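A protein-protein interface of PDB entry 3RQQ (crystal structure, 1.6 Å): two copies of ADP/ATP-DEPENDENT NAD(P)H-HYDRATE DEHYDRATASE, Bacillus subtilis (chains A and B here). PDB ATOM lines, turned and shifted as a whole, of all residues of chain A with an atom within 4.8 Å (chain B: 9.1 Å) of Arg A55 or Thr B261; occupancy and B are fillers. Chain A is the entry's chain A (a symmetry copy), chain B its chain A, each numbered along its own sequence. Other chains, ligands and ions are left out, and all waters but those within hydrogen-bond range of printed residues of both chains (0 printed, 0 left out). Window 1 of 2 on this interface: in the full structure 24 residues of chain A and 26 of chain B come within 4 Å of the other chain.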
ATOM      1  N   LEU A  51      -9.699  21.581  31.992  1.00  0.00           N
ATOM      2  CA  LEU A  51      -8.726  22.650  31.893  1.00  0.00           C
ATOM      3  C   LEU A  51      -7.378  22.065  31.403  1.00  0.00           C
ATOM      4  O   LEU A  51      -6.722  22.606  30.515  1.00  0.00           O
ATOM      5  CB  LEU A  51      -8.524  23.311  33.249  1.00  0.00           C
ATOM      6  CG  LEU A  51      -9.511  24.324  33.724  1.00  0.00           C
ATOM      7  CD1 LEU A  51      -9.329  24.469  35.262  1.00  0.00           C
ATOM      8  CD2 LEU A  51      -9.422  25.702  33.029  1.00  0.00           C
ATOM      9  N   GLY A  52      -6.972  20.928  31.973  1.00  0.00           N
ATOM     10  CA  GLY A  52      -5.749  20.284  31.542  1.00  0.00           C
ATOM     11  C   GLY A  52      -5.761  19.984  30.064  1.00  0.00           C
ATOM     12  O   GLY A  52      -4.786  20.201  29.364  1.00  0.00           O
ATOM     13  N   ALA A  53      -6.870  19.441  29.604  1.00  0.00           N
ATOM     14  CA  ALA A  53      -7.001  19.056  28.197  1.00  0.00           C
ATOM     15  C   ALA A  53      -6.976  20.267  27.263  1.00  0.00           C
ATOM     16  O   ALA A  53      -6.251  20.287  26.261  1.00  0.00           O
ATOM     17  CB  ALA A  53      -8.298  18.215  27.984  1.00  0.00           C
ATOM     18  N   MET A  54      -7.801  21.289  27.547  1.00  0.00           N
ATOM     19  CA  MET A  54      -7.826  22.459  26.660  1.00  0.00           C
ATOM     20  C   MET A  54      -6.539  23.255  26.643  1.00  0.00           C
ATOM     21  O   MET A  54      -6.178  23.898  25.654  1.00  0.00           O
ATOM     22  CB  MET A  54      -9.069  23.338  26.928  1.00  0.00           C
ATOM     23  CG  MET A  54     -10.329  22.579  26.702  1.00  0.00           C
ATOM     24  SD  MET A  54     -11.715  23.634  26.189  1.00  0.00           S
ATOM     25  CE  MET A  54     -11.310  23.878  24.484  1.00  0.00           C
ATOM     26  N   ARG A  55      -5.802  23.214  27.765  1.00  0.00           N
ATOM     27  CA  ARG A  55      -4.495  23.819  27.811  1.00  0.00           C
ATOM     28  C   ARG A  55      -3.466  23.059  26.978  1.00  0.00           C
ATOM     29  O   ARG A  55      -2.398  23.615  26.737  1.00  0.00           O
ATOM     30  CB  ARG A  55      -3.995  23.867  29.260  1.00  0.00           C
ATOM     31  CG  ARG A  55      -4.554  25.009  30.076  1.00  0.00           C
ATOM     32  CD  ARG A  55      -3.916  26.295  29.705  1.00  0.00           C
ATOM     33  NE  ARG A  55      -4.272  27.365  30.651  1.00  0.00           N
ATOM     34  CZ  ARG A  55      -4.307  28.653  30.353  1.00  0.00           C
ATOM     35  NH1 ARG A  55      -4.117  29.069  29.133  1.00  0.00           N
ATOM     36  NH2 ARG A  55      -4.611  29.545  31.278  1.00  0.00           N
ATOM     37  N   SER A  56      -3.758  21.818  26.613  1.00  0.00           N
ATOM     38  CA  SER A  56      -2.726  20.931  26.113  1.00  0.00           C
ATOM     39  C   SER A  56      -2.777  20.660  24.612  1.00  0.00           C
ATOM     40  O   SER A  56      -2.401  19.592  24.129  1.00  0.00           O
ATOM     41  CB  SER A  56      -2.647  19.664  26.971  1.00  0.00           C
ATOM     42  OG  SER A  56      -2.183  19.964  28.277  1.00  0.00           O
ATOM     43  N   GLY A  57      -3.255  21.640  23.825  1.00  0.00           N
ATOM     44  CA  GLY A  57      -3.043  21.599  22.373  1.00  0.00           C
ATOM     45  C   GLY A  57      -4.089  20.942  21.498  1.00  0.00           C
ATOM     46  O   GLY A  57      -3.838  20.821  20.298  1.00  0.00           O
ATOM     47  N   SER A 268      -2.329  23.823  35.421  1.00  0.00           N
ATOM     48  CA  SER A 268      -2.840  24.233  34.118  1.00  0.00           C
ATOM     49  C   SER A 268      -2.535  25.682  33.759  1.00  0.00           C
ATOM     50  O   SER A 268      -2.369  26.001  32.600  1.00  0.00           O
ATOM     51  CB  SER A 268      -4.351  24.014  34.027  1.00  0.00           C
ATOM     52  OG  SER A 268      -4.642  22.681  34.189  1.00  0.00           O
ATOM     53  N   ASP A 269      -2.561  26.544  34.769  1.00  0.00           N
ATOM     54  CA  ASP A 269      -2.324  27.971  34.665  1.00  0.00           C
ATOM     55  C   ASP A 269      -0.796  28.171  34.379  1.00  0.00           C
ATOM     56  O   ASP A 269      -0.401  29.173  33.738  1.00  0.00           O
ATOM     57  CB  ASP A 269      -2.554  28.772  35.988  1.00  0.00           C
ATOM     58  CG  ASP A 269      -4.009  28.856  36.570  1.00  0.00           C
ATOM     59  OD1 ASP A 269      -5.029  28.688  35.864  1.00  0.00           O
ATOM     60  OD2 ASP A 269      -4.090  29.215  37.817  1.00  0.00           O
ATOM     61  N   LEU A 271       1.351  25.812  32.936  1.00  0.00           N
ATOM     62  CA  LEU A 271       1.762  25.079  31.731  1.00  0.00           C
ATOM     63  C   LEU A 271       2.086  25.991  30.540  1.00  0.00           C
ATOM     64  O   LEU A 271       3.032  25.705  29.827  1.00  0.00           O
ATOM     65  CB  LEU A 271       0.727  23.994  31.375  1.00  0.00           C
ATOM     66  CG  LEU A 271       1.030  23.135  30.172  1.00  0.00           C
ATOM     67  CD1 LEU A 271       2.324  22.264  30.358  1.00  0.00           C
ATOM     68  CD2 LEU A 271      -0.143  22.270  29.745  1.00  0.00           C
ATOM     69  N   PRO A 272       1.287  27.062  30.297  1.00  0.00           N
ATOM     70  CA  PRO A 272       1.626  27.949  29.138  1.00  0.00           C
ATOM     71  C   PRO A 272       3.089  28.417  29.103  1.00  0.00           C
ATOM     72  O   PRO A 272       3.727  28.376  28.065  1.00  0.00           O
ATOM     73  CB  PRO A 272       0.656  29.122  29.293  1.00  0.00           C
ATOM     74  CG  PRO A 272      -0.569  28.435  29.899  1.00  0.00           C
ATOM     75  CD  PRO A 272       0.012  27.467  30.913  1.00  0.00           C
ATOM     76  N   TRP A 275       5.674  25.208  28.984  1.00  0.00           N
ATOM     77  CA  TRP A 275       5.745  24.625  27.671  1.00  0.00           C
ATOM     78  C   TRP A 275       6.587  25.500  26.756  1.00  0.00           C
ATOM     79  O   TRP A 275       7.399  25.004  25.991  1.00  0.00           O
ATOM     80  CB  TRP A 275       4.332  24.377  27.147  1.00  0.00           C
ATOM     81  CG  TRP A 275       4.185  23.525  25.909  1.00  0.00           C
ATOM     82  CD1 TRP A 275       5.022  23.432  24.820  1.00  0.00           C
ATOM     83  CD2 TRP A 275       3.046  22.696  25.609  1.00  0.00           C
ATOM     84  NE1 TRP A 275       4.466  22.593  23.874  1.00  0.00           N
ATOM     85  CE2 TRP A 275       3.259  22.140  24.325  1.00  0.00           C
ATOM     86  CE3 TRP A 275       1.881  22.391  26.287  1.00  0.00           C
ATOM     87  CZ2 TRP A 275       2.328  21.277  23.707  1.00  0.00           C
ATOM     88  CZ3 TRP A 275       0.956  21.522  25.683  1.00  0.00           C
ATOM     89  CH2 TRP A 275       1.202  20.969  24.399  1.00  0.00           C
ATOM     90  N   ASN B 209      -1.953  33.691  14.810  1.00  0.00           N
ATOM     91  CA  ASN B 209      -1.150  32.500  14.689  1.00  0.00           C
ATOM     92  C   ASN B 209      -1.950  31.298  15.116  1.00  0.00           C
ATOM     93  O   ASN B 209      -3.169  31.406  15.400  1.00  0.00           O
ATOM     94  CB  ASN B 209       0.158  32.619  15.476  1.00  0.00           C
ATOM     95  CG  ASN B 209      -0.080  32.862  16.934  1.00  0.00           C
ATOM     96  OD1 ASN B 209      -0.948  32.239  17.548  1.00  0.00           O
ATOM     97  ND2 ASN B 209       0.708  33.792  17.530  1.00  0.00           N
ATOM     98  N   GLY B 210      -1.288  30.134  15.124  1.00  0.00           N
ATOM     99  CA  GLY B 210      -1.992  28.895  15.435  1.00  0.00           C
ATOM    100  C   GLY B 210      -2.556  28.760  16.824  1.00  0.00           C
ATOM    101  O   GLY B 210      -3.341  27.829  17.104  1.00  0.00           O
ATOM    102  N   ALA B 211      -2.233  29.687  17.722  1.00  0.00           N
ATOM    103  CA  ALA B 211      -2.829  29.673  19.065  1.00  0.00           C
ATOM    104  C   ALA B 211      -4.324  29.867  18.959  1.00  0.00           C
ATOM    105  O   ALA B 211      -5.089  29.429  19.856  1.00  0.00           O
ATOM    106  CB  ALA B 211      -2.213  30.747  19.986  1.00  0.00           C
ATOM    107  N   LEU B 212      -4.759  30.485  17.860  1.00  0.00           N
ATOM    108  CA  LEU B 212      -6.199  30.731  17.617  1.00  0.00           C
ATOM    109  C   LEU B 212      -6.968  29.517  17.119  1.00  0.00           C
ATOM    110  O   LEU B 212      -8.204  29.535  17.105  1.00  0.00           O
ATOM    111  CB  LEU B 212      -6.379  31.889  16.645  1.00  0.00           C
ATOM    112  CG  LEU B 212      -5.894  33.271  17.075  1.00  0.00           C
ATOM    113  CD1 LEU B 212      -5.943  34.263  15.898  1.00  0.00           C
ATOM    114  CD2 LEU B 212      -6.705  33.783  18.274  1.00  0.00           C
ATOM    115  N   ALA B 213      -6.264  28.457  16.725  1.00  0.00           N
ATOM    116  CA  ALA B 213      -6.906  27.279  16.145  1.00  0.00           C
ATOM    117  C   ALA B 213      -7.412  26.368  17.256  1.00  0.00           C
ATOM    118  O   ALA B 213      -6.919  25.237  17.432  1.00  0.00           O
ATOM    119  CB  ALA B 213      -5.886  26.539  15.228  1.00  0.00           C
ATOM    120  N   LYS B 214      -8.398  26.853  18.001  1.00  0.00           N
ATOM    121  CA  LYS B 214      -8.972  26.141  19.126  1.00  0.00           C
ATOM    122  C   LYS B 214     -10.345  26.698  19.374  1.00  0.00           C
ATOM    123  O   LYS B 214     -10.597  27.913  19.152  1.00  0.00           O
ATOM    124  CB  LYS B 214      -8.084  26.265  20.366  1.00  0.00           C
ATOM    125  CG  LYS B 214      -8.485  25.353  21.493  1.00  0.00           C
ATOM    126  CD  LYS B 214      -7.613  25.479  22.785  1.00  0.00           C
ATOM    127  CE  LYS B 214      -6.106  25.186  22.559  1.00  0.00           C
ATOM    128  NZ  LYS B 214      -5.256  25.572  23.761  1.00  0.00           N
ATOM    129  N   TRP B 253       0.378  36.750  23.260  1.00  0.00           N
ATOM    130  CA  TRP B 253       0.417  35.515  24.041  1.00  0.00           C
ATOM    131  C   TRP B 253       1.632  34.667  23.745  1.00  0.00           C
ATOM    132  O   TRP B 253       2.293  34.168  24.672  1.00  0.00           O
ATOM    133  CB  TRP B 253      -0.819  34.647  23.715  1.00  0.00           C
ATOM    134  CG  TRP B 253      -0.854  33.293  24.356  1.00  0.00           C
ATOM    135  CD1 TRP B 253      -0.585  32.081  23.775  1.00  0.00           C
ATOM    136  CD2 TRP B 253      -1.230  32.995  25.694  1.00  0.00           C
ATOM    137  NE1 TRP B 253      -0.717  31.079  24.686  1.00  0.00           N
ATOM    138  CE2 TRP B 253      -1.152  31.598  25.857  1.00  0.00           C
ATOM    139  CE3 TRP B 253      -1.642  33.771  26.779  1.00  0.00           C
ATOM    140  CZ2 TRP B 253      -1.475  30.975  27.054  1.00  0.00           C
ATOM    141  CZ3 TRP B 253      -1.931  33.169  27.957  1.00  0.00           C
ATOM    142  CH2 TRP B 253      -1.865  31.770  28.097  1.00  0.00           C
ATOM    143  N   THR B 254       1.942  34.477  22.474  1.00  0.00           N
ATOM    144  CA  THR B 254       3.032  33.554  22.114  1.00  0.00           C
ATOM    145  C   THR B 254       4.442  34.092  22.426  1.00  0.00           C
ATOM    146  O   THR B 254       5.422  33.350  22.338  1.00  0.00           O
ATOM    147  CB  THR B 254       2.926  33.029  20.682  1.00  0.00           C
ATOM    148  OG1 THR B 254       2.887  34.139  19.764  1.00  0.00           O
ATOM    149  CG2 THR B 254       1.678  32.179  20.482  1.00  0.00           C
ATOM    150  N   GLU B 256       5.603  34.702  25.374  1.00  0.00           N
ATOM    151  CA  GLU B 256       6.050  34.001  26.554  1.00  0.00           C
ATOM    152  C   GLU B 256       5.261  32.764  26.928  1.00  0.00           C
ATOM    153  O   GLU B 256       5.546  32.154  27.951  1.00  0.00           O
ATOM    154  CB  GLU B 256       6.039  34.947  27.719  1.00  0.00           C
ATOM    155  CG  GLU B 256       6.948  36.175  27.524  1.00  0.00           C
ATOM    156  CD  GLU B 256       7.158  36.889  28.818  1.00  0.00           C
ATOM    157  OE1 GLU B 256       6.226  37.564  29.290  1.00  0.00           O
ATOM    158  OE2 GLU B 256       8.249  36.743  29.376  1.00  0.00           O
ATOM    159  N   HIS B 257       4.308  32.408  26.093  1.00  0.00           N
ATOM    160  CA  HIS B 257       3.464  31.238  26.302  1.00  0.00           C
ATOM    161  C   HIS B 257       3.427  30.376  25.047  1.00  0.00           C
ATOM    162  O   HIS B 257       3.436  30.880  23.927  1.00  0.00           O
ATOM    163  CB  HIS B 257       2.036  31.621  26.660  1.00  0.00           C
ATOM    164  CG  HIS B 257       1.904  32.667  27.713  1.00  0.00           C
ATOM    165  ND1 HIS B 257       2.000  34.022  27.441  1.00  0.00           N
ATOM    166  CD2 HIS B 257       1.724  32.565  29.056  1.00  0.00           C
ATOM    167  CE1 HIS B 257       1.867  34.709  28.564  1.00  0.00           C
ATOM    168  NE2 HIS B 257       1.658  33.855  29.565  1.00  0.00           N
ATOM    169  N   SER B 258       3.332  29.064  25.189  1.00  0.00           N
ATOM    170  CA  SER B 258       3.198  28.211  24.024  1.00  0.00           C
ATOM    171  C   SER B 258       1.900  28.426  23.278  1.00  0.00           C
ATOM    172  O   SER B 258       0.802  28.511  23.881  1.00  0.00           O
ATOM    173  CB  SER B 258       3.294  26.727  24.455  1.00  0.00           C
ATOM    174  OG  SER B 258       2.907  25.896  23.367  1.00  0.00           O
ATOM    175  N   ALA B 259       1.993  28.476  21.938  1.00  0.00           N
ATOM    176  CA  ALA B 259       0.821  28.569  21.119  1.00  0.00           C
ATOM    177  C   ALA B 259      -0.179  27.423  21.293  1.00  0.00           C
ATOM    178  O   ALA B 259      -1.333  27.594  20.954  1.00  0.00           O
ATOM    179  CB  ALA B 259       1.237  28.653  19.631  1.00  0.00           C
ATOM    180  N   HIS B 260       0.225  26.276  21.825  1.00  0.00           N
ATOM    181  CA  HIS B 260      -0.711  25.181  22.076  1.00  0.00           C
ATOM    182  C   HIS B 260      -1.636  25.404  23.248  1.00  0.00           C
ATOM    183  O   HIS B 260      -2.609  24.682  23.399  1.00  0.00           O
ATOM    184  CB  HIS B 260       0.064  23.898  22.373  1.00  0.00           C
ATOM    185  CG  HIS B 260       0.790  23.368  21.194  1.00  0.00           C
ATOM    186  ND1 HIS B 260       0.142  22.861  20.080  1.00  0.00           N
ATOM    187  CD2 HIS B 260       2.112  23.255  20.964  1.00  0.00           C
ATOM    188  CE1 HIS B 260       1.065  22.415  19.232  1.00  0.00           C
ATOM    189  NE2 HIS B 260       2.259  22.669  19.731  1.00  0.00           N
ATOM    190  N   THR B 261      -1.390  26.442  24.052  1.00  0.00           N
ATOM    191  CA  THR B 261      -1.972  26.517  25.406  1.00  0.00           C
ATOM    192  C   THR B 261      -2.942  27.676  25.642  1.00  0.00           C
ATOM    193  O   THR B 261      -3.487  27.772  26.722  1.00  0.00           O
ATOM    194  CB  THR B 261      -0.861  26.602  26.477  1.00  0.00           C
ATOM    195  OG1 THR B 261      -0.173  27.891  26.390  1.00  0.00           O
ATOM    196  CG2 THR B 261       0.182  25.474  26.323  1.00  0.00           C
ATOM    197  N   LEU B 262      -3.198  28.513  24.647  1.00  0.00           N
ATOM    198  CA  LEU B 262      -4.107  29.630  24.804  1.00  0.00           C
ATOM    199  C   LEU B 262      -5.558  29.168  24.982  1.00  0.00           C
ATOM    200  O   LEU B 262      -6.004  28.259  24.278  1.00  0.00           O
ATOM    201  CB  LEU B 262      -4.061  30.511  23.539  1.00  0.00           C
ATOM    202  CG  LEU B 262      -4.969  31.754  23.525  1.00  0.00           C
ATOM    203  CD1 LEU B 262      -4.660  32.818  24.594  1.00  0.00           C
ATOM    204  CD2 LEU B 262      -4.947  32.370  22.099  1.00  0.00           C
ATOM    205  N   LEU B 263      -6.268  29.806  25.882  1.00  0.00           N
ATOM    206  CA  LEU B 263      -7.720  29.657  25.967  1.00  0.00           C
ATOM    207  C   LEU B 263      -8.364  30.931  25.437  1.00  0.00           C
ATOM    208  O   LEU B 263      -7.928  32.023  25.758  1.00  0.00           O
ATOM    209  CB  LEU B 263      -8.160  29.390  27.409  1.00  0.00           C
ATOM    210  CG  LEU B 263      -7.518  28.156  28.026  1.00  0.00           C
ATOM    211  CD1 LEU B 263      -7.865  28.017  29.509  1.00  0.00           C
ATOM    212  CD2 LEU B 263      -7.955  26.870  27.261  1.00  0.00           C
ATOM    213  N   ALA B 264      -9.414  30.827  24.624  1.00  0.00           N
ATOM    214  CA  ALA B 264     -10.016  31.983  23.975  1.00  0.00           C
ATOM    215  C   ALA B 264     -10.314  33.158  24.896  1.00  0.00           C
ATOM    216  O   ALA B 264     -10.105  34.302  24.496  1.00  0.00           O
ATOM    217  CB  ALA B 264     -11.355  31.552  23.290  1.00  0.00           C
ATOM    218  N   HIS B 265     -10.848  32.893  26.097  1.00  0.00           N
ATOM    219  CA  HIS B 265     -11.213  34.021  26.984  1.00  0.00           C
ATOM    220  C   HIS B 265     -10.024  34.894  27.301  1.00  0.00           C
ATOM    221  O   HIS B 265     -10.177  36.073  27.625  1.00  0.00           O
ATOM    222  CB  HIS B 265     -11.929  33.578  28.233  1.00  0.00           C
ATOM    223  CG  HIS B 265     -11.118  32.775  29.197  1.00  0.00           C
ATOM    224  ND1 HIS B 265     -10.382  33.326  30.233  1.00  0.00           N
ATOM    225  CD2 HIS B 265     -10.929  31.441  29.270  1.00  0.00           C
ATOM    226  CE1 HIS B 265      -9.766  32.354  30.886  1.00  0.00           C
ATOM    227  NE2 HIS B 265     -10.103  31.200  30.346  1.00  0.00           N
ATOM    228  N   GLU B 266      -8.816  34.328  27.253  1.00  0.00           N
ATOM    229  CA  GLU B 266      -7.632  35.075  27.552  1.00  0.00           C
ATOM    230  C   GLU B 266      -7.365  36.139  26.501  1.00  0.00           C
ATOM    231  O   GLU B 266      -6.689  37.167  26.773  1.00  0.00           O
ATOM    232  CB  GLU B 266      -6.447  34.124  27.718  1.00  0.00           C
ATOM    233  CG  GLU B 266      -6.615  33.251  28.937  1.00  0.00           C
ATOM    234  CD  GLU B 266      -5.563  32.205  29.104  1.00  0.00           C
ATOM    235  OE1 GLU B 266      -5.265  31.459  28.158  1.00  0.00           O
ATOM    236  OE2 GLU B 266      -5.028  32.166  30.287  1.00  0.00           O
ATOM    237  N   LEU B 267      -7.868  35.964  25.276  1.00  0.00           N
ATOM    238  CA  LEU B 267      -7.695  36.989  24.271  1.00  0.00           C
ATOM    239  C   LEU B 267      -8.343  38.310  24.756  1.00  0.00           C
ATOM    240  O   LEU B 267      -7.751  39.408  24.591  1.00  0.00           O
ATOM    241  CB  LEU B 267      -8.313  36.592  22.963  1.00  0.00           C
ATOM    242  CG  LEU B 267      -7.670  35.426  22.210  1.00  0.00           C
ATOM    243  CD1 LEU B 267      -8.675  34.907  21.141  1.00  0.00           C
ATOM    244  CD2 LEU B 267      -6.361  35.869  21.573  1.00  0.00           C
ATOM    245  N   ASP B 269      -8.721  39.184  27.905  1.00  0.00           N
ATOM    246  CA  ASP B 269      -7.937  39.592  29.055  1.00  0.00           C
ATOM    247  C   ASP B 269      -6.682  40.362  28.515  1.00  0.00           C
ATOM    248  O   ASP B 269      -6.139  41.250  29.213  1.00  0.00           O
ATOM    249  CB  ASP B 269      -7.316  38.415  29.876  1.00  0.00           C
ATOM    250  CG  ASP B 269      -8.283  37.438  30.633  1.00  0.00           C
ATOM    251  OD1 ASP B 269      -9.449  37.760  30.959  1.00  0.00           O
ATOM    252  OD2 ASP B 269      -7.759  36.305  30.994  1.00  0.00           O
ATOM    253  N   ILE B 270      -6.164  39.980  27.326  1.00  0.00           N
ATOM    254  CA  ILE B 270      -4.952  40.582  26.709  1.00  0.00           C
ATOM    255  C   ILE B 270      -5.218  41.870  25.961  1.00  0.00           C
ATOM    256  O   ILE B 270      -4.397  42.786  25.885  1.00  0.00           O
ATOM    257  CB  ILE B 270      -4.295  39.518  25.711  1.00  0.00           C
ATOM    258  CG1 ILE B 270      -3.757  38.400  26.576  1.00  0.00           C
ATOM    259  CG2 ILE B 270      -3.204  40.116  24.799  1.00  0.00           C
ATOM    260  CD1 ILE B 270      -3.476  37.128  25.775  1.00  0.00           C
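N of His B260 lies close to OG of Ser B258, 3.1 Å away. OE1 of Glu B266 is in hydrogen-bond range of N of Leu B263, 3.0 Å away. The backbone carbonyl oxygen (O) of Ser B258 lies within hydrogen-bond range of the side-chain hydroxyl (OG1) of Thr B261, at 2.8 Å. O of His B260 sits at hydrogen-bond distance from NZ of Lys B214. The side-chain amino group of Lys B214 lies within hydrogen-bond range of the backbone carbonyl oxygen of Leu B262 (2.8 Å). O of Trp B253 is in hydrogen-bond range of ND1 of His B257.
No residue of chain B comes within 4 Å of Gly A52. Arg A55 touches five residues of chain B. No residue of chain B comes within 4 Å of Ser A56. Pro A272 touches just these residues of chain B: Trp B253 (3.6 Å), His B257 (3.4 Å), Ser B258 (3.0 Å) and Thr B261 (3.3 Å). Of the printed residues of chain A, Lys B214 touches Met A54. Of the printed residues of chain A, Trp B253 touches Arg A55 (3.7 Å) and Pro A272 (3.6 Å). Printed residues of chain A within 4 Å of Ser B258: Pro A272 and Trp A275. Of the printed residues of chain A, His B260 touches Arg A55 (3.5 Å), Gly A57 (3.1 Å) and Trp A275 (3.4 Å). Thr B261 touches three residues of chain A. Ala B264 touches none of the printed residues of chain A. The nearest residue of chain B that does not touch Arg A55 is Leu B262 (4.4 Å). The nearest residue of chain A that does not touch Thr B261 is Leu A271 (4.5 Å).
Position printed for both chains: 269. Of the 15 pairs that touch across the chains among the printed residues, none has its exchanged pair printed and touching as well.
Printed residues of chain B that touch a printed residue of chain A: Lys B214, Trp B253, His B257, Ser B258, His B260, Thr B261, Leu B263 and Glu B266. Printed residues of chain A that touch a printed residue of chain B: Met A54, Arg A55, Gly A57, Pro A272 and Trp A275. Hydrophobic or aromatic side chains of chain A that line the printed part of chain B: Met A54, Pro A272 and Trp A275. Along chain A the printed residues that touch a printed residue of chain B span positions 54 to 275. Among the printed residues, 15 pairs touch across the chains.
N of Ser B258 lies within hydrogen-bond range of O of Pro A272 (3.0 Å). The side-chain carboxylate (OE1) of Glu B266 is in salt-bridge range of the guanidinium group (NH1) of Arg A55, 2.8 Å away. The backbone carbonyl oxygen (O) of Thr B261 sits at hydrogen-bond distance from the guanidinium group (NH1) of Arg A55, 2.8 Å away. O of Met A54 lies within hydrogen-bond range of NZ of Lys B214, at 2.7 Å. O of His B260 sits at hydrogen-bond distance from N of Gly A57.
Met A54 touches Leu B263 (CB to CD2, 3.7 Å). Arg A55 touches Trp B253. Arg A55 touches His B260 (O to O, 3.5 Å). Arg A55 touches Leu B263. Pro A272 touches Trp B253 (CB to CZ2, 3.6 Å). O of Pro A272 touches CA of His B257, 3.4 Å away. Pro A272 touches Thr B261. OG of Ser B258 touches CD1 of Trp A275, 3.6 Å away. CZ2 of Trp A275 touches CD2 of His B260, at 3.4 Å. CE3 of Trp A275 touches CG2 of Thr B261 (3.5 Å).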
